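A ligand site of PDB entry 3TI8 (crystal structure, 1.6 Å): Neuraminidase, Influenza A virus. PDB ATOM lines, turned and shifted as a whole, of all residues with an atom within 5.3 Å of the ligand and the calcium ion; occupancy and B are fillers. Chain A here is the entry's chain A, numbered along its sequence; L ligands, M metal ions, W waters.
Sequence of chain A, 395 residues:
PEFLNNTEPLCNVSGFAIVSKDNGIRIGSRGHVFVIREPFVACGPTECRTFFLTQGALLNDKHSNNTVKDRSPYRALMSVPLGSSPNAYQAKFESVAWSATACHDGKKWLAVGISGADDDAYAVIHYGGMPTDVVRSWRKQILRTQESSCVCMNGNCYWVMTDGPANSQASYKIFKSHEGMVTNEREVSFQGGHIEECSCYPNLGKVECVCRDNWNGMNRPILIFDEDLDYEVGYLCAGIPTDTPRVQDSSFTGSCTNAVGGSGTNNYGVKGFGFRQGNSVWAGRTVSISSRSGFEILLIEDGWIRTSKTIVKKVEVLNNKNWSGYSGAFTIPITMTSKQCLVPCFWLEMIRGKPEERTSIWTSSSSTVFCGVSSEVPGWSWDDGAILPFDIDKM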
ATOM      1  N   ARG A  37      -4.137 -15.246   3.614  1.00  0.00           N
ATOM      2  CA  ARG A  37      -4.868 -16.184   2.756  1.00  0.00           C
ATOM      3  C   ARG A  37      -6.243 -15.576   2.532  1.00  0.00           C
ATOM      4  O   ARG A  37      -6.519 -14.485   3.033  1.00  0.00           O
ATOM      5  CB  ARG A  37      -4.966 -17.592   3.357  1.00  0.00           C
ATOM      6  CG  ARG A  37      -4.010 -18.623   2.734  1.00  0.00           C
ATOM      7  CD  ARG A  37      -4.611 -20.023   2.734  1.00  0.00           C
ATOM      8  NE  ARG A  37      -5.784 -20.078   1.846  1.00  0.00           N
ATOM      9  CZ  ARG A  37      -6.796 -20.918   1.970  1.00  0.00           C
ATOM     10  NH1 ARG A  37      -6.824 -21.821   2.950  1.00  0.00           N
ATOM     11  NH2 ARG A  37      -7.812 -20.847   1.108  1.00  0.00           N
ATOM     12  N   GLU A  38      -7.078 -16.248   1.764  1.00  0.00           N
ATOM     13  CA  GLU A  38      -8.423 -15.749   1.497  1.00  0.00           C
ATOM     14  C   GLU A  38      -8.427 -14.312   0.939  1.00  0.00           C
ATOM     15  O   GLU A  38      -9.118 -13.436   1.451  1.00  0.00           O
ATOM     16  CB  GLU A  38      -9.288 -15.834   2.757  1.00  0.00           C
ATOM     17  CG  GLU A  38      -9.469 -17.265   3.304  1.00  0.00           C
ATOM     18  CD  GLU A  38      -8.345 -17.719   4.230  1.00  0.00           C
ATOM     19  OE1 GLU A  38      -8.097 -18.950   4.288  1.00  0.00           O
ATOM     20  OE2 GLU A  38      -7.721 -16.872   4.901  1.00  0.00           O
ATOM     21  N   LEU A  53      -7.046 -11.604   4.294  1.00  0.00           N
ATOM     22  CA  LEU A  53      -6.933 -11.879   5.716  1.00  0.00           C
ATOM     23  C   LEU A  53      -5.468 -12.116   6.059  1.00  0.00           C
ATOM     24  O   LEU A  53      -4.894 -13.135   5.672  1.00  0.00           O
ATOM     25  CB  LEU A  53      -7.750 -13.105   6.110  1.00  0.00           C
ATOM     26  CG  LEU A  53      -9.265 -13.014   5.889  1.00  0.00           C
ATOM     27  CD1 LEU A  53      -9.947 -14.302   6.334  1.00  0.00           C
ATOM     28  CD2 LEU A  53      -9.856 -11.807   6.619  1.00  0.00           C
ATOM     29  N   ASP A  70      -6.316 -21.656  10.632  1.00  0.00           N
ATOM     30  CA  ASP A  70      -7.346 -20.809  10.049  1.00  0.00           C
ATOM     31  C   ASP A  70      -7.748 -19.578  10.849  1.00  0.00           C
ATOM     32  O   ASP A  70      -8.061 -18.531  10.272  1.00  0.00           O
ATOM     33  CB  ASP A  70      -8.598 -21.627   9.753  1.00  0.00           C
ATOM     34  CG  ASP A  70      -8.471 -22.451   8.503  1.00  0.00           C
ATOM     35  OD1 ASP A  70      -8.104 -21.884   7.453  1.00  0.00           O
ATOM     36  OD2 ASP A  70      -8.740 -23.670   8.560  1.00  0.00           O
ATOM     37  N   ARG A  71      -7.764 -19.694  12.176  1.00  0.00           N
ATOM     38  CA  ARG A  71      -8.345 -18.651  13.012  1.00  0.00           C
ATOM     39  C   ARG A  71      -7.436 -18.301  14.192  1.00  0.00           C
ATOM     40  O   ARG A  71      -6.895 -19.186  14.842  1.00  0.00           O
ATOM     41  CB  ARG A  71      -9.753 -19.052  13.490  1.00  0.00           C
ATOM     42  CG  ARG A  71     -10.703 -19.391  12.337  1.00  0.00           C
ATOM     43  CD  ARG A  71     -12.073 -19.913  12.798  1.00  0.00           C
ATOM     44  NE  ARG A  71     -11.970 -21.134  13.602  1.00  0.00           N
ATOM     45  CZ  ARG A  71     -11.754 -22.343  13.090  1.00  0.00           C
ATOM     46  NH1 ARG A  71     -11.623 -22.513  11.783  1.00  0.00           N
ATOM     47  NH2 ARG A  71     -11.670 -23.391  13.908  1.00  0.00           N
ATOM     48  N   ARG A  75      -5.426 -12.275  13.144  1.00  0.00           N
ATOM     49  CA  ARG A  75      -5.830 -12.095  11.754  1.00  0.00           C
ATOM     50  C   ARG A  75      -6.657 -10.835  11.572  1.00  0.00           C
ATOM     51  O   ARG A  75      -7.507 -10.507  12.398  1.00  0.00           O
ATOM     52  CB  ARG A  75      -6.588 -13.326  11.240  1.00  0.00           C
ATOM     53  CG  ARG A  75      -5.822 -14.629  11.408  1.00  0.00           C
ATOM     54  CD  ARG A  75      -6.276 -15.671  10.377  1.00  0.00           C
ATOM     55  NE  ARG A  75      -5.867 -15.331   9.012  1.00  0.00           N
ATOM     56  CZ  ARG A  75      -6.057 -16.119   7.951  1.00  0.00           C
ATOM     57  NH1 ARG A  75      -6.675 -17.289   8.093  1.00  0.00           N
ATOM     58  NH2 ARG A  75      -5.649 -15.726   6.749  1.00  0.00           N
ATOM     59  N   TRP A  98     -11.044 -13.177  10.972  1.00  0.00           N
ATOM     60  CA  TRP A  98     -10.576 -14.439  10.404  1.00  0.00           C
ATOM     61  C   TRP A  98     -11.566 -14.983   9.352  1.00  0.00           C
ATOM     62  O   TRP A  98     -11.355 -16.049   8.783  1.00  0.00           O
ATOM     63  CB  TRP A  98     -10.212 -15.493  11.462  1.00  0.00           C
ATOM     64  CG  TRP A  98     -11.132 -15.666  12.659  1.00  0.00           C
ATOM     65  CD1 TRP A  98     -10.845 -15.343  13.955  1.00  0.00           C
ATOM     66  CD2 TRP A  98     -12.439 -16.275  12.673  1.00  0.00           C
ATOM     67  NE1 TRP A  98     -11.898 -15.684  14.780  1.00  0.00           N
ATOM     68  CE2 TRP A  98     -12.884 -16.256  14.021  1.00  0.00           C
ATOM     69  CE3 TRP A  98     -13.265 -16.809  11.689  1.00  0.00           C
ATOM     70  CZ2 TRP A  98     -14.135 -16.760  14.395  1.00  0.00           C
ATOM     71  CZ3 TRP A  98     -14.506 -17.313  12.072  1.00  0.00           C
ATOM     72  CH2 TRP A  98     -14.923 -17.282  13.408  1.00  0.00           C
ATOM     73  N   SER A  99     -12.617 -14.215   9.085  1.00  0.00           N
ATOM     74  CA  SER A  99     -13.521 -14.468   7.972  1.00  0.00           C
ATOM     75  C   SER A  99     -14.162 -13.132   7.619  1.00  0.00           C
ATOM     76  O   SER A  99     -14.434 -12.330   8.504  1.00  0.00           O
ATOM     77  CB  SER A  99     -14.600 -15.496   8.350  1.00  0.00           C
ATOM     78  OG  SER A  99     -15.481 -15.728   7.264  1.00  0.00           O
ATOM     79  N   ILE A 142     -18.555 -21.460  14.791  1.00  0.00           N
ATOM     80  CA  ILE A 142     -17.726 -20.834  13.759  1.00  0.00           C
ATOM     81  C   ILE A 142     -18.549 -20.049  12.733  1.00  0.00           C
ATOM     82  O   ILE A 142     -18.614 -20.404  11.547  1.00  0.00           O
ATOM     83  CB  ILE A 142     -16.780 -21.852  13.081  1.00  0.00           C
ATOM     84  CG1 ILE A 142     -16.070 -22.705  14.134  1.00  0.00           C
ATOM     85  CG2 ILE A 142     -15.746 -21.111  12.219  1.00  0.00           C
ATOM     86  CD1 ILE A 142     -15.138 -23.751  13.541  1.00  0.00           C
ATOM     87  N   LEU A 143     -19.184 -18.987  13.202  1.00  0.00           N
ATOM     88  CA  LEU A 143     -19.820 -18.025  12.320  1.00  0.00           C
ATOM     89  C   LEU A 143     -18.829 -17.669  11.216  1.00  0.00           C
ATOM     90  O   LEU A 143     -17.671 -17.372  11.494  1.00  0.00           O
ATOM     91  CB  LEU A 143     -20.207 -16.771  13.102  1.00  0.00           C
ATOM     92  CG  LEU A 143     -20.811 -15.598  12.337  1.00  0.00           C
ATOM     93  CD1 LEU A 143     -22.170 -15.959  11.739  1.00  0.00           C
ATOM     94  CD2 LEU A 143     -20.932 -14.403  13.265  1.00  0.00           C
ATOM     95  N   ARG A 144     -19.274 -17.709   9.975  1.00  0.00           N
ATOM     96  CA  ARG A 144     -18.356 -17.489   8.855  1.00  0.00           C
ATOM     97  C   ARG A 144     -19.076 -16.920   7.638  1.00  0.00           C
ATOM     98  O   ARG A 144     -20.291 -17.027   7.520  1.00  0.00           O
ATOM     99  CB  ARG A 144     -17.620 -18.778   8.506  1.00  0.00           C
ATOM    100  CG  ARG A 144     -18.517 -19.999   8.312  1.00  0.00           C
ATOM    101  CD  ARG A 144     -17.714 -21.274   8.524  1.00  0.00           C
ATOM    102  NE  ARG A 144     -18.432 -22.507   8.193  1.00  0.00           N
ATOM    103  CZ  ARG A 144     -19.245 -23.155   9.019  1.00  0.00           C
ATOM    104  NH1 ARG A 144     -19.476 -22.680  10.245  1.00  0.00           N
ATOM    105  NH2 ARG A 144     -19.833 -24.282   8.626  1.00  0.00           N
ATOM    106  N   GLU A 147     -15.682 -14.644   2.202  1.00  0.00           N
ATOM    107  CA  GLU A 147     -14.297 -14.480   1.740  1.00  0.00           C
ATOM    108  C   GLU A 147     -14.248 -13.972   0.290  1.00  0.00           C
ATOM    109  O   GLU A 147     -13.329 -14.290  -0.476  1.00  0.00           O
ATOM    110  CB  GLU A 147     -13.461 -15.774   1.858  1.00  0.00           C
ATOM    111  CG  GLU A 147     -13.834 -16.692   3.019  1.00  0.00           C
ATOM    112  CD  GLU A 147     -13.674 -16.064   4.377  1.00  0.00           C
ATOM    113  OE1 GLU A 147     -13.243 -14.895   4.469  1.00  0.00           O
ATOM    114  OE2 GLU A 147     -13.977 -16.751   5.378  1.00  0.00           O
ATOM    115  N   ALA A 166     -19.182 -28.121   9.964  1.00  0.00           N
ATOM    116  CA  ALA A 166     -18.465 -28.066   8.695  1.00  0.00           C
ATOM    117  C   ALA A 166     -18.842 -29.235   7.788  1.00  0.00           C
ATOM    118  O   ALA A 166     -18.780 -29.114   6.571  1.00  0.00           O
ATOM    119  CB  ALA A 166     -16.955 -28.074   8.940  1.00  0.00           C
ATOM    120  N   GLU A 196     -21.346 -22.585   1.996  1.00  0.00           N
ATOM    121  CA  GLU A 196     -20.255 -21.818   2.564  1.00  0.00           C
ATOM    122  C   GLU A 196     -19.603 -20.946   1.512  1.00  0.00           C
ATOM    123  O   GLU A 196     -19.688 -21.235   0.314  1.00  0.00           O
ATOM    124  CB  GLU A 196     -19.169 -22.747   3.138  1.00  0.00           C
ATOM    125  CG  GLU A 196     -19.616 -23.617   4.276  1.00  0.00           C
ATOM    126  CD  GLU A 196     -18.474 -24.393   4.875  1.00  0.00           C
ATOM    127  OE1 GLU A 196     -18.486 -24.609   6.101  1.00  0.00           O
ATOM    128  OE2 GLU A 196     -17.562 -24.782   4.110  1.00  0.00           O
ATOM    129  N   GLU A 197     -18.958 -19.877   1.949  1.00  0.00           N
ATOM    130  CA  GLU A 197     -18.059 -19.108   1.102  1.00  0.00           C
ATOM    131  C   GLU A 197     -18.665 -18.751  -0.252  1.00  0.00           C
ATOM    132  O   GLU A 197     -18.070 -18.978  -1.306  1.00  0.00           O
ATOM    133  CB  GLU A 197     -16.745 -19.874   0.933  1.00  0.00           C
ATOM    134  CG  GLU A 197     -15.991 -20.015   2.254  1.00  0.00           C
ATOM    135  CD  GLU A 197     -14.768 -20.911   2.167  1.00  0.00           C
ATOM    136  OE1 GLU A 197     -14.691 -21.758   1.252  1.00  0.00           O
ATOM    137  OE2 GLU A 197     -13.885 -20.764   3.045  1.00  0.00           O
ATOM    138  N   ARG A 212     -19.892 -23.119  -1.860  1.00  0.00           N
ATOM    139  CA  ARG A 212     -19.177 -24.345  -1.557  1.00  0.00           C
ATOM    140  C   ARG A 212     -20.040 -25.219  -0.650  1.00  0.00           C
ATOM    141  O   ARG A 212     -20.537 -24.757   0.366  1.00  0.00           O
ATOM    142  CB  ARG A 212     -17.858 -24.016  -0.856  1.00  0.00           C
ATOM    143  CG  ARG A 212     -17.173 -25.168  -0.112  1.00  0.00           C
ATOM    144  CD  ARG A 212     -15.960 -24.631   0.663  1.00  0.00           C
ATOM    145  NE  ARG A 212     -15.253 -25.625   1.462  1.00  0.00           N
ATOM    146  CZ  ARG A 212     -14.048 -25.417   1.996  1.00  0.00           C
ATOM    147  NH1 ARG A 212     -13.419 -24.263   1.786  1.00  0.00           N
ATOM    148  NH2 ARG A 212     -13.460 -26.357   2.726  1.00  0.00           N
ATOM    149  N   ASP A 213     -20.212 -26.485  -1.037  1.00  0.00           N
ATOM    150  CA  ASP A 213     -20.871 -27.464  -0.181  1.00  0.00           C
ATOM    151  C   ASP A 213     -19.768 -28.288   0.445  1.00  0.00           C
ATOM    152  O   ASP A 213     -19.024 -28.951  -0.262  1.00  0.00           O
ATOM    153  CB  ASP A 213     -21.809 -28.337  -1.038  1.00  0.00           C
ATOM    154  CG  ASP A 213     -22.515 -29.421  -0.232  1.00  0.00           C
ATOM    155  OD1 ASP A 213     -21.852 -30.127   0.552  1.00  0.00           O
ATOM    156  OD2 ASP A 213     -23.747 -29.585  -0.405  1.00  0.00           O
ATOM    157  N   ASN A 214     -19.621 -28.238   1.767  1.00  0.00           N
ATOM    158  CA  ASN A 214     -18.536 -28.936   2.442  1.00  0.00           C
ATOM    159  C   ASN A 214     -18.994 -30.252   3.072  1.00  0.00           C
ATOM    160  O   ASN A 214     -18.300 -30.837   3.912  1.00  0.00           O
ATOM    161  CB  ASN A 214     -17.923 -28.034   3.532  1.00  0.00           C
ATOM    162  CG  ASN A 214     -16.460 -28.318   3.768  1.00  0.00           C
ATOM    163  OD1 ASN A 214     -15.641 -28.250   2.851  1.00  0.00           O
ATOM    164  ND2 ASN A 214     -16.113 -28.639   5.012  1.00  0.00           N
ATOM    165  N   TRP A 215     -20.166 -30.713   2.632  1.00  0.00           N
ATOM    166  CA  TRP A 215     -20.838 -31.864   3.224  1.00  0.00           C
ATOM    167  C   TRP A 215     -20.954 -32.959   2.166  1.00  0.00           C
ATOM    168  O   TRP A 215     -19.981 -33.644   1.870  1.00  0.00           O
ATOM    169  CB  TRP A 215     -22.204 -31.416   3.745  1.00  0.00           C
ATOM    170  CG  TRP A 215     -23.008 -32.454   4.480  1.00  0.00           C
ATOM    171  CD1 TRP A 215     -22.577 -33.666   4.946  1.00  0.00           C
ATOM    172  CD2 TRP A 215     -24.392 -32.356   4.852  1.00  0.00           C
ATOM    173  NE1 TRP A 215     -23.615 -34.325   5.568  1.00  0.00           N
ATOM    174  CE2 TRP A 215     -24.737 -33.541   5.529  1.00  0.00           C
ATOM    175  CE3 TRP A 215     -25.368 -31.372   4.673  1.00  0.00           C
ATOM    176  CZ2 TRP A 215     -26.013 -33.773   6.019  1.00  0.00           C
ATOM    177  CZ3 TRP A 215     -26.638 -31.601   5.156  1.00  0.00           C
ATOM    178  CH2 TRP A 215     -26.953 -32.784   5.829  1.00  0.00           C
ATOM    179  N   GLY A 217     -21.878 -32.633  -1.235  1.00  0.00           N
ATOM    180  CA  GLY A 217     -21.927 -32.212  -2.629  1.00  0.00           C
ATOM    181  C   GLY A 217     -20.599 -31.857  -3.264  1.00  0.00           C
ATOM    182  O   GLY A 217     -19.846 -31.033  -2.736  1.00  0.00           O
ATOM    183  N   MET A 218     -20.298 -32.466  -4.403  1.00  0.00           N
ATOM    184  CA  MET A 218     -19.138 -32.078  -5.213  1.00  0.00           C
ATOM    185  C   MET A 218     -19.615 -31.125  -6.318  1.00  0.00           C
ATOM    186  O   MET A 218     -18.802 -30.588  -7.073  1.00  0.00           O
ATOM    187  CB  MET A 218     -18.448 -33.297  -5.828  1.00  0.00           C
ATOM    188  CG  MET A 218     -19.191 -33.887  -7.020  1.00  0.00           C
ATOM    189  SD  MET A 218     -18.362 -35.311  -7.748  1.00  0.00           S
ATOM    190  CE  MET A 218     -19.041 -36.644  -6.754  1.00  0.00           C
ATOM    191  N   ASP A 243     -16.550 -28.449  -7.848  1.00  0.00           N
ATOM    192  CA  ASP A 243     -15.922 -28.358  -6.529  1.00  0.00           C
ATOM    193  C   ASP A 243     -14.635 -29.175  -6.565  1.00  0.00           C
ATOM    194  O   ASP A 243     -14.364 -29.850  -7.553  1.00  0.00           O
ATOM    195  CB  ASP A 243     -16.868 -28.913  -5.460  1.00  0.00           C
ATOM    196  CG  ASP A 243     -16.512 -28.450  -4.052  1.00  0.00           C
ATOM    197  OD1 ASP A 243     -15.604 -27.616  -3.876  1.00  0.00           O
ATOM    198  OD2 ASP A 243     -17.181 -28.932  -3.109  1.00  0.00           O
ATOM    199  N   PRO A 245     -12.644 -31.654  -3.549  1.00  0.00           N
ATOM    200  CA  PRO A 245     -12.533 -32.783  -4.480  1.00  0.00           C
ATOM    201  C   PRO A 245     -13.811 -33.107  -5.242  1.00  0.00           C
ATOM    202  O   PRO A 245     -14.904 -32.717  -4.846  1.00  0.00           O
ATOM    203  CB  PRO A 245     -12.167 -33.956  -3.563  1.00  0.00           C
ATOM    204  CG  PRO A 245     -12.797 -33.618  -2.261  1.00  0.00           C
ATOM    205  CD  PRO A 245     -12.683 -32.109  -2.147  1.00  0.00           C
ATOM    206  N   THR A 265     -15.413 -37.897  -2.135  1.00  0.00           N
ATOM    207  CA  THR A 265     -15.456 -36.451  -2.304  1.00  0.00           C
ATOM    208  C   THR A 265     -16.167 -35.724  -1.165  1.00  0.00           C
ATOM    209  O   THR A 265     -16.132 -34.492  -1.088  1.00  0.00           O
ATOM    210  CB  THR A 265     -16.128 -36.049  -3.636  1.00  0.00           C
ATOM    211  OG1 THR A 265     -17.545 -36.282  -3.552  1.00  0.00           O
ATOM    212  CG2 THR A 265     -15.544 -36.834  -4.797  1.00  0.00           C
ATOM    213  N   TYR A 268     -15.380 -32.156   2.176  1.00  0.00           N
ATOM    214  CA  TYR A 268     -14.432 -31.078   1.897  1.00  0.00           C
ATOM    215  C   TYR A 268     -14.934 -30.303   0.698  1.00  0.00           C
ATOM    216  O   TYR A 268     -16.043 -30.517   0.225  1.00  0.00           O
ATOM    217  CB  TYR A 268     -13.013 -31.608   1.668  1.00  0.00           C
ATOM    218  CG  TYR A 268     -11.915 -30.593   1.951  1.00  0.00           C
ATOM    219  CD1 TYR A 268     -11.913 -29.854   3.140  1.00  0.00           C
ATOM    220  CD2 TYR A 268     -10.875 -30.389   1.061  1.00  0.00           C
ATOM    221  CE1 TYR A 268     -10.915 -28.939   3.415  1.00  0.00           C
ATOM    222  CE2 TYR A 268      -9.865 -29.467   1.322  1.00  0.00           C
ATOM    223  CZ  TYR A 268      -9.893 -28.750   2.503  1.00  0.00           C
ATOM    224  OH  TYR A 268      -8.897 -27.832   2.792  1.00  0.00           O
ATOM    225  N   GLY A 269     -14.122 -29.366   0.223  1.00  0.00           N
ATOM    226  CA  GLY A 269     -14.528 -28.498  -0.864  1.00  0.00           C
ATOM    227  C   GLY A 269     -13.533 -27.372  -0.970  1.00  0.00           C
ATOM    228  O   GLY A 269     -12.525 -27.343  -0.258  1.00  0.00           O
ATOM    229  N   ARG A 292      -5.844 -28.857  -4.767  1.00  0.00           N
ATOM    230  CA  ARG A 292      -5.968 -27.472  -5.200  1.00  0.00           C
ATOM    231  C   ARG A 292      -4.781 -27.105  -6.096  1.00  0.00           C
ATOM    232  O   ARG A 292      -3.878 -26.372  -5.699  1.00  0.00           O
ATOM    233  CB  ARG A 292      -6.054 -26.553  -3.980  1.00  0.00           C
ATOM    234  CG  ARG A 292      -7.311 -26.823  -3.147  1.00  0.00           C
ATOM    235  CD  ARG A 292      -7.285 -26.167  -1.774  1.00  0.00           C
ATOM    236  NE  ARG A 292      -8.578 -26.331  -1.112  1.00  0.00           N
ATOM    237  CZ  ARG A 292      -8.927 -25.726   0.028  1.00  0.00           C
ATOM    238  NH1 ARG A 292      -8.069 -24.932   0.654  1.00  0.00           N
ATOM    239  NH2 ARG A 292     -10.134 -25.932   0.545  1.00  0.00           N
ATOM    240  N   TYR A 326      -8.536 -20.897  -3.496  1.00  0.00           N
ATOM    241  CA  TYR A 326      -9.832 -20.240  -3.629  1.00  0.00           C
ATOM    242  C   TYR A 326      -9.955 -19.455  -4.930  1.00  0.00           C
ATOM    243  O   TYR A 326      -8.957 -19.024  -5.505  1.00  0.00           O
ATOM    244  CB  TYR A 326     -10.063 -19.297  -2.447  1.00  0.00           C
ATOM    245  CG  TYR A 326     -10.496 -19.988  -1.180  1.00  0.00           C
ATOM    246  CD1 TYR A 326     -10.416 -21.376  -1.047  1.00  0.00           C
ATOM    247  CD2 TYR A 326     -10.992 -19.262  -0.100  1.00  0.00           C
ATOM    248  CE1 TYR A 326     -10.831 -22.016   0.108  1.00  0.00           C
ATOM    249  CE2 TYR A 326     -11.403 -19.895   1.061  1.00  0.00           C
ATOM    250  CZ  TYR A 326     -11.321 -21.270   1.146  1.00  0.00           C
ATOM    251  OH  TYR A 326     -11.736 -21.909   2.301  1.00  0.00           O
HETATM  252  C1  LIG L   1     -10.668 -23.256   4.604  1.00  0.00           C
HETATM  253  C2  LIG L   1     -10.135 -21.843   4.818  1.00  0.00           C
HETATM  254  C3  LIG L   1     -10.869 -20.981   5.855  1.00  0.00           C
HETATM  255  C4  LIG L   1     -12.134 -21.604   6.504  1.00  0.00           C
HETATM  256  C5  LIG L   1     -12.717 -22.890   5.870  1.00  0.00           C
HETATM  257  O1  LIG L   1     -12.015 -23.550   4.839  1.00  0.00           O
HETATM  258  C6  LIG L   1     -10.004 -24.148   3.607  1.00  0.00           C
HETATM  259  O2  LIG L   1      -8.831 -23.730   3.056  1.00  0.00           O
HETATM  260  O3  LIG L   1     -10.689 -24.988   3.042  1.00  0.00           O
HETATM  261  C7  LIG L   1     -13.583 -23.787   6.694  1.00  0.00           C
HETATM  262  C8  LIG L   1     -14.512 -24.612   5.813  1.00  0.00           C
HETATM  263  C9  LIG L   1     -15.423 -25.508   6.615  1.00  0.00           C
HETATM  264  O4  LIG L   1     -16.314 -24.861   7.485  1.00  0.00           O
HETATM  265  O5  LIG L   1     -12.786 -24.524   7.529  1.00  0.00           O
HETATM  266  C10 LIG L   1     -12.969 -24.418   8.901  1.00  0.00           C
HETATM  267  O6  LIG L   1     -15.159 -23.848   4.865  1.00  0.00           O
HETATM  268  N1  LIG L   1     -10.072 -20.080   6.637  1.00  0.00           N
HETATM  269  C11 LIG L   1     -10.509 -18.773   7.045  1.00  0.00           C
HETATM  270  N2  LIG L   1      -9.783 -18.162   7.957  1.00  0.00           N
HETATM  271  N3  LIG L   1     -11.512 -18.164   6.420  1.00  0.00           N
HETATM  272  C12 LIG L   1     -12.799 -20.480   8.683  1.00  0.00           C
HETATM  273  C13 LIG L   1     -13.736 -19.494   9.297  1.00  0.00           C
HETATM  274  O7  LIG L   1     -11.913 -21.036   9.336  1.00  0.00           O
HETATM  275  N4  LIG L   1     -13.009 -20.793   7.316  1.00  0.00           N
HETATM  276 CA    CA M   1     -17.789 -30.539  -1.502  1.00  0.00          CA
HETATM  277  O   HOH W   1      -7.304 -23.884   5.693  1.00  0.00           O
HETATM  278  O   HOH W   2      -9.987 -25.314   7.149  1.00  0.00           O
HETATM  279  O   HOH W   3     -11.521 -26.479   5.673  1.00  0.00           O
HETATM  280  O   HOH W   4     -16.381 -32.294  -2.600  1.00  0.00           O
HETATM  281  O   HOH W   5     -18.531 -32.584  -0.278  1.00  0.00           O
HETATM  282  O   HOH W   6      -8.688 -26.906   5.170  1.00  0.00           O
HETATM  283  O   HOH W   7     -14.425 -26.593  11.096  1.00  0.00           O
HETATM  284  O   HOH W   8     -14.142 -19.384   5.297  1.00  0.00           O
HETATM  285  O   HOH W   9     -16.175 -24.660  10.190  1.00  0.00           O
HETATM  286  O   HOH W  10     -16.403 -21.277   5.564  1.00  0.00           O
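Water W4 lies within hydrogen-bond range of O of Thr 265 (2.7 Å) and O of Pro 245 (2.7 Å).
Water W5 lies within hydrogen-bond range of the backbone carbonyl oxygen (O) of Trp 215 (2.8 Å), the backbone carbonyl oxygen (O) of Thr 265 (3.2 Å) and the backbone NH (N) of Gly 217 (3.5 Å).
Water W8 lies within hydrogen-bond range of OE2 of Glu 147 (2.6 Å), OE2 of Glu 197 (2.7 Å) and N4 of the ligand (2.7 Å).
Water W2 bridges OD2 of Asp 70 (2.5 Å) and O5 of the ligand (2.9 Å).
Water W1 lies within hydrogen-bond range of the side-chain carboxylate of Asp 70 (2.8 Å), an oxygen (O2) of the ligand (3.1 Å) and the guanidinium group of Arg 37 (3.5 Å).
Water W6 bridges OH of Tyr 268 (2.6 Å) and O3 of the ligand (3.5 Å).
N of Asp 243 lies close to O of Met 218 (3.2 Å).
NH2 of Arg 75 lies within salt-bridge range of OE2 of Glu 38, at 3.0 Å.
The guanidinium group of Arg 212 is in hydrogen-bond range of the side-chain hydroxyl of Tyr 326.
The side-chain carboxylate (OD1) of Asp 213 lies within hydrogen-bond range of the backbone NH (N) of Gly 217 (3.1 Å).
NH1 of Arg 212 lies within salt-bridge range of OE1 of Glu 197.
O of Asp 70 sits at hydrogen-bond distance from NH1 of Arg 75 (2.9 Å).
NH2 of Arg 212 sits at hydrogen-bond distance from OD1 of Asn 214 (2.9 Å).
The guanidinium group (NH1) of Arg 144 is in hydrogen-bond range of the backbone carbonyl oxygen (O) of Ile 142 (2.8 Å).
The guanidinium group (NE) of Arg 144 is in hydrogen-bond range of an oxygen (O4) of the ligand.
The backbone carbonyl oxygen (O) of Asp 70 is in hydrogen-bond range of a nitrogen (N2) of the ligand, 2.9 Å away.
The backbone carbonyl oxygen (O) of Trp 98 is in hydrogen-bond range of a nitrogen (N2) of the ligand, at 2.8 Å.
The side-chain carboxylate (OE2) of Glu 147 is in salt-bridge range of a nitrogen (N3) of the ligand, 3.0 Å away.
NH2 of Arg 292 lies within salt-bridge range of O3 of the ligand.
The side-chain carboxylate of Glu 196 lies within hydrogen-bond range of an oxygen (O4) of the ligand, at 2.6 Å.
The side-chain carboxylate (OD1) of Asp 70 lies within salt-bridge range of a nitrogen (N1) of the ligand (2.8 Å).
The side-chain hydroxyl (OH) of Tyr 326 lies close to an oxygen (O1) of the ligand (3.0 Å).
An oxygen (O3) of the ligand is in salt-bridge range of the guanidinium group (NH1) of Arg 212 (3.1 Å).
NH1 of Arg 37 lies within salt-bridge range of O2 of the ligand (2.8 Å).
The side-chain hydroxyl (OH) of Tyr 268 is in hydrogen-bond range of an oxygen (O3) of the ligand.
An oxygen (O7) of the ligand sits at hydrogen-bond distance from the guanidinium group (NH1) of Arg 71 (2.9 Å).
OE1 of Glu 38 is in salt-bridge range of N1 of the ligand (3.3 Å).
CA of Gly 269 touches the calcium ion (3.9 Å).
Within 4 Å of the calcium ion: Asp 213, Gly 217, Asp 243, Tyr 268 and Gly 269.
OD2 of Asp 243 is bound to the calcium ion, 2.4 Å away.
O of Asp 213 is bound to the calcium ion, at 2.4 Å.
The calcium ion is bound by O of Gly 217.
The calcium ion is bound by O of Tyr 268, at 2.5 Å.
Water W5 is bound to the calcium ion (2.5 Å).
Water W4 binds the calcium ion, at 2.5 Å.
The calcium ion has six donor atoms within binding distance.
A nitrogen (N2) of the ligand sits close to the guanidinium group of Arg 75 (3.2 Å).
Ile 142 touches the ligand (CG2 to C13, 3.9 Å).
Ala 166 touches the ligand (CB to O4, 3.6 Å).
OE2 of Glu 197 touches C5 of the ligand, 3.7 Å away.
Asn 214 touches the ligand (ND2 to C9, 3.6 Å).
Hydrophobic or aromatic side chains that line the ligand: Trp 98, Ile 142, Ala 166, Tyr 268 and Tyr 326.
The nearest printed residue that does not touch the ligand is Leu 53 (4.2 Å).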
